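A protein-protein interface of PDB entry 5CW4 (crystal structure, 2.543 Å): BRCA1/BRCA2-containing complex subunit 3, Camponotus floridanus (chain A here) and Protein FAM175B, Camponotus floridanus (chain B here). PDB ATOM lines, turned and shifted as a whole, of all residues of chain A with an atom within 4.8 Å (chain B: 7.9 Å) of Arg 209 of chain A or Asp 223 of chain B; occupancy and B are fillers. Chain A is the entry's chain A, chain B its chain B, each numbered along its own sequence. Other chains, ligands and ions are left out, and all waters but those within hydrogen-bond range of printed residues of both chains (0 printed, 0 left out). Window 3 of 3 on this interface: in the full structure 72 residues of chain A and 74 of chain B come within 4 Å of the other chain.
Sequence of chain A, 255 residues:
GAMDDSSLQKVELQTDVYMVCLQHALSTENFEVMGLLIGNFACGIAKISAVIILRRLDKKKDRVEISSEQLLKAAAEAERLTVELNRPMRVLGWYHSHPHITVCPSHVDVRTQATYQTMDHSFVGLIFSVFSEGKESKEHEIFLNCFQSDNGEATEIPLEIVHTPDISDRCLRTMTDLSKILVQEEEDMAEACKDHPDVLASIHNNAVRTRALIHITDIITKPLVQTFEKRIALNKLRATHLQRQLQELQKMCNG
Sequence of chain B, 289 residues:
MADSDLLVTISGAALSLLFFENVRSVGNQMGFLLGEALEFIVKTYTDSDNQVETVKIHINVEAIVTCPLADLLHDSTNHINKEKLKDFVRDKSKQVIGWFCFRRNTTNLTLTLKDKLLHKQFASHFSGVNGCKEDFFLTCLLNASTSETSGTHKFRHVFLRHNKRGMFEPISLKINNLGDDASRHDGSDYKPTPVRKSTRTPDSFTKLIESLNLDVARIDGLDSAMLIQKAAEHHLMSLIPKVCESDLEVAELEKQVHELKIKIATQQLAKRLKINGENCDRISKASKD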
ATOM      1  N   GLU A 187     -13.891   2.317  14.847  1.00  0.00           N
ATOM      2  CA  GLU A 187     -13.536   1.150  14.049  1.00  0.00           C
ATOM      3  C   GLU A 187     -12.027   1.031  13.866  1.00  0.00           C
ATOM      4  O   GLU A 187     -11.463  -0.054  14.022  1.00  0.00           O
ATOM      5  CB  GLU A 187     -14.221   1.208  12.684  1.00  0.00           C
ATOM      6  CG  GLU A 187     -15.720   1.045  12.743  1.00  0.00           C
ATOM      7  CD  GLU A 187     -16.127  -0.311  13.272  1.00  0.00           C
ATOM      8  OE1 GLU A 187     -15.482  -1.313  12.898  1.00  0.00           O
ATOM      9  OE2 GLU A 187     -17.089  -0.375  14.067  1.00  0.00           O
ATOM     10  N   ALA A 190     -10.370  -0.075  17.193  1.00  0.00           N
ATOM     11  CA  ALA A 190     -10.678  -1.473  17.472  1.00  0.00           C
ATOM     12  C   ALA A 190      -9.993  -2.390  16.460  1.00  0.00           C
ATOM     13  O   ALA A 190      -9.655  -3.531  16.773  1.00  0.00           O
ATOM     14  CB  ALA A 190     -12.189  -1.697  17.469  1.00  0.00           C
ATOM     15  N   ASN A 205     -12.114  -6.207  24.801  1.00  0.00           N
ATOM     16  CA  ASN A 205     -12.130  -5.307  23.652  1.00  0.00           C
ATOM     17  C   ASN A 205     -13.510  -5.184  23.018  1.00  0.00           C
ATOM     18  O   ASN A 205     -13.934  -4.085  22.651  1.00  0.00           O
ATOM     19  CB  ASN A 205     -11.117  -5.762  22.604  1.00  0.00           C
ATOM     20  CG  ASN A 205      -9.685  -5.533  23.043  1.00  0.00           C
ATOM     21  OD1 ASN A 205      -9.388  -4.564  23.747  1.00  0.00           O
ATOM     22  ND2 ASN A 205      -8.787  -6.425  22.632  1.00  0.00           N
ATOM     23  N   ASN A 206     -14.210  -6.308  22.893  1.00  0.00           N
ATOM     24  CA  ASN A 206     -15.583  -6.294  22.398  1.00  0.00           C
ATOM     25  C   ASN A 206     -16.497  -5.471  23.301  1.00  0.00           C
ATOM     26  O   ASN A 206     -17.324  -4.696  22.822  1.00  0.00           O
ATOM     27  CB  ASN A 206     -16.117  -7.717  22.264  1.00  0.00           C
ATOM     28  CG  ASN A 206     -15.411  -8.501  21.179  1.00  0.00           C
ATOM     29  OD1 ASN A 206     -15.038  -7.950  20.146  1.00  0.00           O
ATOM     30  ND2 ASN A 206     -15.220  -9.794  21.410  1.00  0.00           N
ATOM     31  N   ALA A 207     -16.335  -5.634  24.609  1.00  0.00           N
ATOM     32  CA  ALA A 207     -17.100  -4.848  25.567  1.00  0.00           C
ATOM     33  C   ALA A 207     -16.835  -3.358  25.368  1.00  0.00           C
ATOM     34  O   ALA A 207     -17.761  -2.545  25.375  1.00  0.00           O
ATOM     35  CB  ALA A 207     -16.768  -5.268  26.989  1.00  0.00           C
ATOM     36  N   VAL A 208     -15.568  -3.006  25.173  1.00  0.00           N
ATOM     37  CA  VAL A 208     -15.189  -1.612  24.962  1.00  0.00           C
ATOM     38  C   VAL A 208     -15.787  -1.068  23.664  1.00  0.00           C
ATOM     39  O   VAL A 208     -16.323   0.042  23.631  1.00  0.00           O
ATOM     40  CB  VAL A 208     -13.654  -1.447  24.933  1.00  0.00           C
ATOM     41  CG1 VAL A 208     -13.269  -0.058  24.452  1.00  0.00           C
ATOM     42  CG2 VAL A 208     -13.061  -1.725  26.308  1.00  0.00           C
ATOM     43  N   ARG A 209     -15.704  -1.862  22.601  1.00  0.00           N
ATOM     44  CA  ARG A 209     -16.187  -1.442  21.294  1.00  0.00           C
ATOM     45  C   ARG A 209     -17.703  -1.259  21.283  1.00  0.00           C
ATOM     46  O   ARG A 209     -18.217  -0.285  20.727  1.00  0.00           O
ATOM     47  CB  ARG A 209     -15.772  -2.453  20.216  1.00  0.00           C
ATOM     48  CG  ARG A 209     -16.021  -1.966  18.792  1.00  0.00           C
ATOM     49  CD  ARG A 209     -15.535  -2.972  17.752  1.00  0.00           C
ATOM     50  NE  ARG A 209     -16.643  -3.735  17.187  1.00  0.00           N
ATOM     51  CZ  ARG A 209     -17.300  -3.383  16.087  1.00  0.00           C
ATOM     52  NH1 ARG A 209     -16.947  -2.287  15.433  1.00  0.00           N
ATOM     53  NH2 ARG A 209     -18.303  -4.127  15.637  1.00  0.00           N
ATOM     54  N   THR A 210     -18.416  -2.198  21.894  1.00  0.00           N
ATOM     55  CA  THR A 210     -19.875  -2.142  21.925  1.00  0.00           C
ATOM     56  C   THR A 210     -20.361  -0.919  22.702  1.00  0.00           C
ATOM     57  O   THR A 210     -21.311  -0.256  22.294  1.00  0.00           O
ATOM     58  CB  THR A 210     -20.474  -3.423  22.538  1.00  0.00           C
ATOM     59  OG1 THR A 210     -20.163  -4.541  21.697  1.00  0.00           O
ATOM     60  CG2 THR A 210     -21.985  -3.304  22.673  1.00  0.00           C
ATOM     61  N   ARG A 211     -19.697  -0.617  23.812  1.00  0.00           N
ATOM     62  CA  ARG A 211     -20.054   0.544  24.619  1.00  0.00           C
ATOM     63  C   ARG A 211     -19.772   1.867  23.903  1.00  0.00           C
ATOM     64  O   ARG A 211     -20.545   2.823  24.015  1.00  0.00           O
ATOM     65  CB  ARG A 211     -19.307   0.526  25.951  1.00  0.00           C
ATOM     66  CG  ARG A 211     -19.515   1.798  26.751  1.00  0.00           C
ATOM     67  CD  ARG A 211     -18.608   1.875  27.956  1.00  0.00           C
ATOM     68  NE  ARG A 211     -18.904   3.052  28.764  1.00  0.00           N
ATOM     69  CZ  ARG A 211     -18.416   3.264  29.979  1.00  0.00           C
ATOM     70  NH1 ARG A 211     -17.602   2.372  30.529  1.00  0.00           N
ATOM     71  NH2 ARG A 211     -18.745   4.362  30.647  1.00  0.00           N
ATOM     72  N   ALA A 212     -18.656   1.930  23.184  1.00  0.00           N
ATOM     73  CA  ALA A 212     -18.299   3.147  22.465  1.00  0.00           C
ATOM     74  C   ALA A 212     -19.265   3.405  21.314  1.00  0.00           C
ATOM     75  O   ALA A 212     -19.676   4.541  21.084  1.00  0.00           O
ATOM     76  CB  ALA A 212     -16.874   3.064  21.951  1.00  0.00           C
ATOM     77  N   LEU A 213     -19.625   2.348  20.592  1.00  0.00           N
ATOM     78  CA  LEU A 213     -20.546   2.478  19.469  1.00  0.00           C
ATOM     79  C   LEU A 213     -21.938   2.883  19.946  1.00  0.00           C
ATOM     80  O   LEU A 213     -22.537   3.816  19.408  1.00  0.00           O
ATOM     81  CB  LEU A 213     -20.617   1.173  18.672  1.00  0.00           C
ATOM     82  CG  LEU A 213     -19.381   0.842  17.831  1.00  0.00           C
ATOM     83  CD1 LEU A 213     -19.550  -0.496  17.127  1.00  0.00           C
ATOM     84  CD2 LEU A 213     -19.098   1.947  16.820  1.00  0.00           C
ATOM     85  N   LEU B 214     -34.292  -5.500  15.219  1.00  0.00           N
ATOM     86  CA  LEU B 214     -32.930  -5.295  15.711  1.00  0.00           C
ATOM     87  C   LEU B 214     -32.808  -5.309  17.236  1.00  0.00           C
ATOM     88  O   LEU B 214     -31.700  -5.331  17.777  1.00  0.00           O
ATOM     89  CB  LEU B 214     -32.367  -3.975  15.180  1.00  0.00           C
ATOM     90  CG  LEU B 214     -31.830  -3.970  13.748  1.00  0.00           C
ATOM     91  CD1 LEU B 214     -31.371  -2.576  13.371  1.00  0.00           C
ATOM     92  CD2 LEU B 214     -30.693  -4.963  13.604  1.00  0.00           C
ATOM     93  N   VAL B 216     -32.935  -7.495  19.235  1.00  0.00           N
ATOM     94  CA  VAL B 216     -32.530  -8.810  19.725  1.00  0.00           C
ATOM     95  C   VAL B 216     -31.176  -9.238  19.150  1.00  0.00           C
ATOM     96  O   VAL B 216     -30.834  -8.889  18.019  1.00  0.00           O
ATOM     97  CB  VAL B 216     -33.583  -9.877  19.385  1.00  0.00           C
ATOM     98  CG1 VAL B 216     -33.153 -11.236  19.913  1.00  0.00           C
ATOM     99  CG2 VAL B 216     -34.935  -9.482  19.954  1.00  0.00           C
ATOM    100  N   ALA B 217     -30.412  -9.992  19.937  1.00  0.00           N
ATOM    101  CA  ALA B 217     -29.103 -10.487  19.514  1.00  0.00           C
ATOM    102  C   ALA B 217     -28.484 -11.376  20.591  1.00  0.00           C
ATOM    103  O   ALA B 217     -27.834 -10.885  21.516  1.00  0.00           O
ATOM    104  CB  ALA B 217     -28.171  -9.328  19.184  1.00  0.00           C
ATOM    105  N   GLY B 221     -25.631 -12.857  18.924  1.00  0.00           N
ATOM    106  CA  GLY B 221     -24.254 -12.605  18.538  1.00  0.00           C
ATOM    107  C   GLY B 221     -24.161 -11.994  17.153  1.00  0.00           C
ATOM    108  O   GLY B 221     -23.397 -12.459  16.304  1.00  0.00           O
ATOM    109  N   LEU B 222     -24.944 -10.943  16.932  1.00  0.00           N
ATOM    110  CA  LEU B 222     -25.043 -10.298  15.626  1.00  0.00           C
ATOM    111  C   LEU B 222     -24.148  -9.068  15.494  1.00  0.00           C
ATOM    112  O   LEU B 222     -23.851  -8.632  14.379  1.00  0.00           O
ATOM    113  CB  LEU B 222     -26.496  -9.892  15.349  1.00  0.00           C
ATOM    114  CG  LEU B 222     -27.442 -10.927  14.744  1.00  0.00           C
ATOM    115  CD1 LEU B 222     -27.071 -11.187  13.296  1.00  0.00           C
ATOM    116  CD2 LEU B 222     -27.422 -12.216  15.555  1.00  0.00           C
ATOM    117  N   ASP B 223     -23.718  -8.528  16.632  1.00  0.00           N
ATOM    118  CA  ASP B 223     -23.116  -7.197  16.705  1.00  0.00           C
ATOM    119  C   ASP B 223     -24.234  -6.171  16.563  1.00  0.00           C
ATOM    120  O   ASP B 223     -24.341  -5.470  15.554  1.00  0.00           O
ATOM    121  CB  ASP B 223     -22.036  -6.991  15.636  1.00  0.00           C
ATOM    122  CG  ASP B 223     -21.294  -5.674  15.799  1.00  0.00           C
ATOM    123  OD1 ASP B 223     -21.399  -5.059  16.883  1.00  0.00           O
ATOM    124  OD2 ASP B 223     -20.599  -5.259  14.848  1.00  0.00           O
ATOM    125  N   SER B 224     -25.070  -6.106  17.593  1.00  0.00           N
ATOM    126  CA  SER B 224     -26.272  -5.288  17.579  1.00  0.00           C
ATOM    127  C   SER B 224     -25.971  -3.795  17.504  1.00  0.00           C
ATOM    128  O   SER B 224     -26.701  -3.043  16.857  1.00  0.00           O
ATOM    129  CB  SER B 224     -27.115  -5.582  18.821  1.00  0.00           C
ATOM    130  OG  SER B 224     -26.414  -5.224  20.000  1.00  0.00           O
ATOM    131  N   ALA B 225     -24.909  -3.364  18.177  1.00  0.00           N
ATOM    132  CA  ALA B 225     -24.563  -1.949  18.209  1.00  0.00           C
ATOM    133  C   ALA B 225     -24.342  -1.424  16.796  1.00  0.00           C
ATOM    134  O   ALA B 225     -24.885  -0.384  16.416  1.00  0.00           O
ATOM    135  CB  ALA B 225     -23.323  -1.711  19.063  1.00  0.00           C
ATOM    136  N   MET B 226     -23.554  -2.159  16.016  1.00  0.00           N
ATOM    137  CA  MET B 226     -23.232  -1.746  14.657  1.00  0.00           C
ATOM    138  C   MET B 226     -24.461  -1.789  13.756  1.00  0.00           C
ATOM    139  O   MET B 226     -24.693  -0.870  12.968  1.00  0.00           O
ATOM    140  CB  MET B 226     -22.124  -2.626  14.074  1.00  0.00           C
ATOM    141  CG  MET B 226     -21.550  -2.099  12.768  1.00  0.00           C
ATOM    142  SD  MET B 226     -20.856  -0.272  12.919  1.00  0.00           S
ATOM    143  CE  MET B 226     -20.045  -0.105  11.155  1.00  0.00           C
ATOM    144  N   LEU B 227     -25.244  -2.857  13.880  1.00  0.00           N
ATOM    145  CA  LEU B 227     -26.460  -3.023  13.091  1.00  0.00           C
ATOM    146  C   LEU B 227     -27.487  -1.925  13.379  1.00  0.00           C
ATOM    147  O   LEU B 227     -28.162  -1.446  12.469  1.00  0.00           O
ATOM    148  CB  LEU B 227     -27.073  -4.402  13.346  1.00  0.00           C
ATOM    149  CG  LEU B 227     -26.206  -5.590  12.917  1.00  0.00           C
ATOM    150  CD1 LEU B 227     -26.867  -6.919  13.263  1.00  0.00           C
ATOM    151  CD2 LEU B 227     -25.891  -5.514  11.428  1.00  0.00           C
ATOM    152  N   ILE B 228     -27.602  -1.527  14.642  1.00  0.00           N
ATOM    153  CA  ILE B 228     -28.509  -0.444  15.020  1.00  0.00           C
ATOM    154  C   ILE B 228     -28.025   0.892  14.461  1.00  0.00           C
ATOM    155  O   ILE B 228     -28.803   1.655  13.891  1.00  0.00           O
ATOM    156  CB  ILE B 228     -28.656  -0.337  16.549  1.00  0.00           C
ATOM    157  CG1 ILE B 228     -29.460  -1.528  17.082  1.00  0.00           C
ATOM    158  CG2 ILE B 228     -29.317   0.981  16.938  1.00  0.00           C
ATOM    159  CD1 ILE B 228     -29.481  -1.629  18.590  1.00  0.00           C
ATOM    160  N   GLN B 229     -26.733   1.159  14.614  1.00  0.00           N
ATOM    161  CA  GLN B 229     -26.133   2.381  14.088  1.00  0.00           C
ATOM    162  C   GLN B 229     -26.319   2.515  12.577  1.00  0.00           C
ATOM    163  O   GLN B 229     -26.696   3.581  12.086  1.00  0.00           O
ATOM    164  CB  GLN B 229     -24.644   2.434  14.430  1.00  0.00           C
ATOM    165  CG  GLN B 229     -23.886   3.530  13.704  1.00  0.00           C
ATOM    166  CD  GLN B 229     -24.379   4.922  14.060  1.00  0.00           C
ATOM    167  OE1 GLN B 229     -24.982   5.132  15.115  1.00  0.00           O
ATOM    168  NE2 GLN B 229     -24.124   5.882  13.175  1.00  0.00           N
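NH2 of Arg 209 of chain A lies within salt-bridge range of OD2 of Asp 223 of chain B (2.7 Å).
Of the 12 printed residues of chain B, 3 touch a printed residue of chain A.
Printed residues of chain B that touch a printed residue of chain A: Asp 223, Ala 225 and Met 226.
Hydrophobic or aromatic side chains of chain B that line the printed part of chain A: Ala 225 and Met 226.
Among the printed residues, Asp or Glu carboxylates within 4 Å of a Lys or Arg side-chain nitrogen of the other chain: Arg 209 of chain A with Asp 223 of chain B.
Asp 223 of chain B touches just one residue of chain A: Arg 209 (2.7 Å).
Of the printed residues of chain A, Met 226 of chain B touches Glu 187 (3.9 Å).
Of the printed residues of chain B, Leu 213 of chain A touches Ala 225 (3.97 Å).
Of the printed residues of chain A, Ala 225 of chain B touches Leu 213 (3.97 Å).
Asn 205 of chain A touches none of the printed residues of chain B.
Leu 214 of chain B touches none of the printed residues of chain A.
The nearest printed residue of chain A that does not touch Asp 223 of chain B is Leu 213 of chain A (4.9 Å).
The nearest printed residue of chain B that does not touch Glu 187 of chain A is Asp 223 of chain B (6.1 Å).
Among the printed residues, pairs that only touch across the chains: Glu 187 of chain A with Met 226 of chain B and Leu 213 of chain A with Ala 225 of chain B.
The side-chain carboxylate (OE1) of Glu 187 of chain A is in salt-bridge range of the guanidinium group (NH1) of Arg 209 of chain A, at 3.1 Å.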
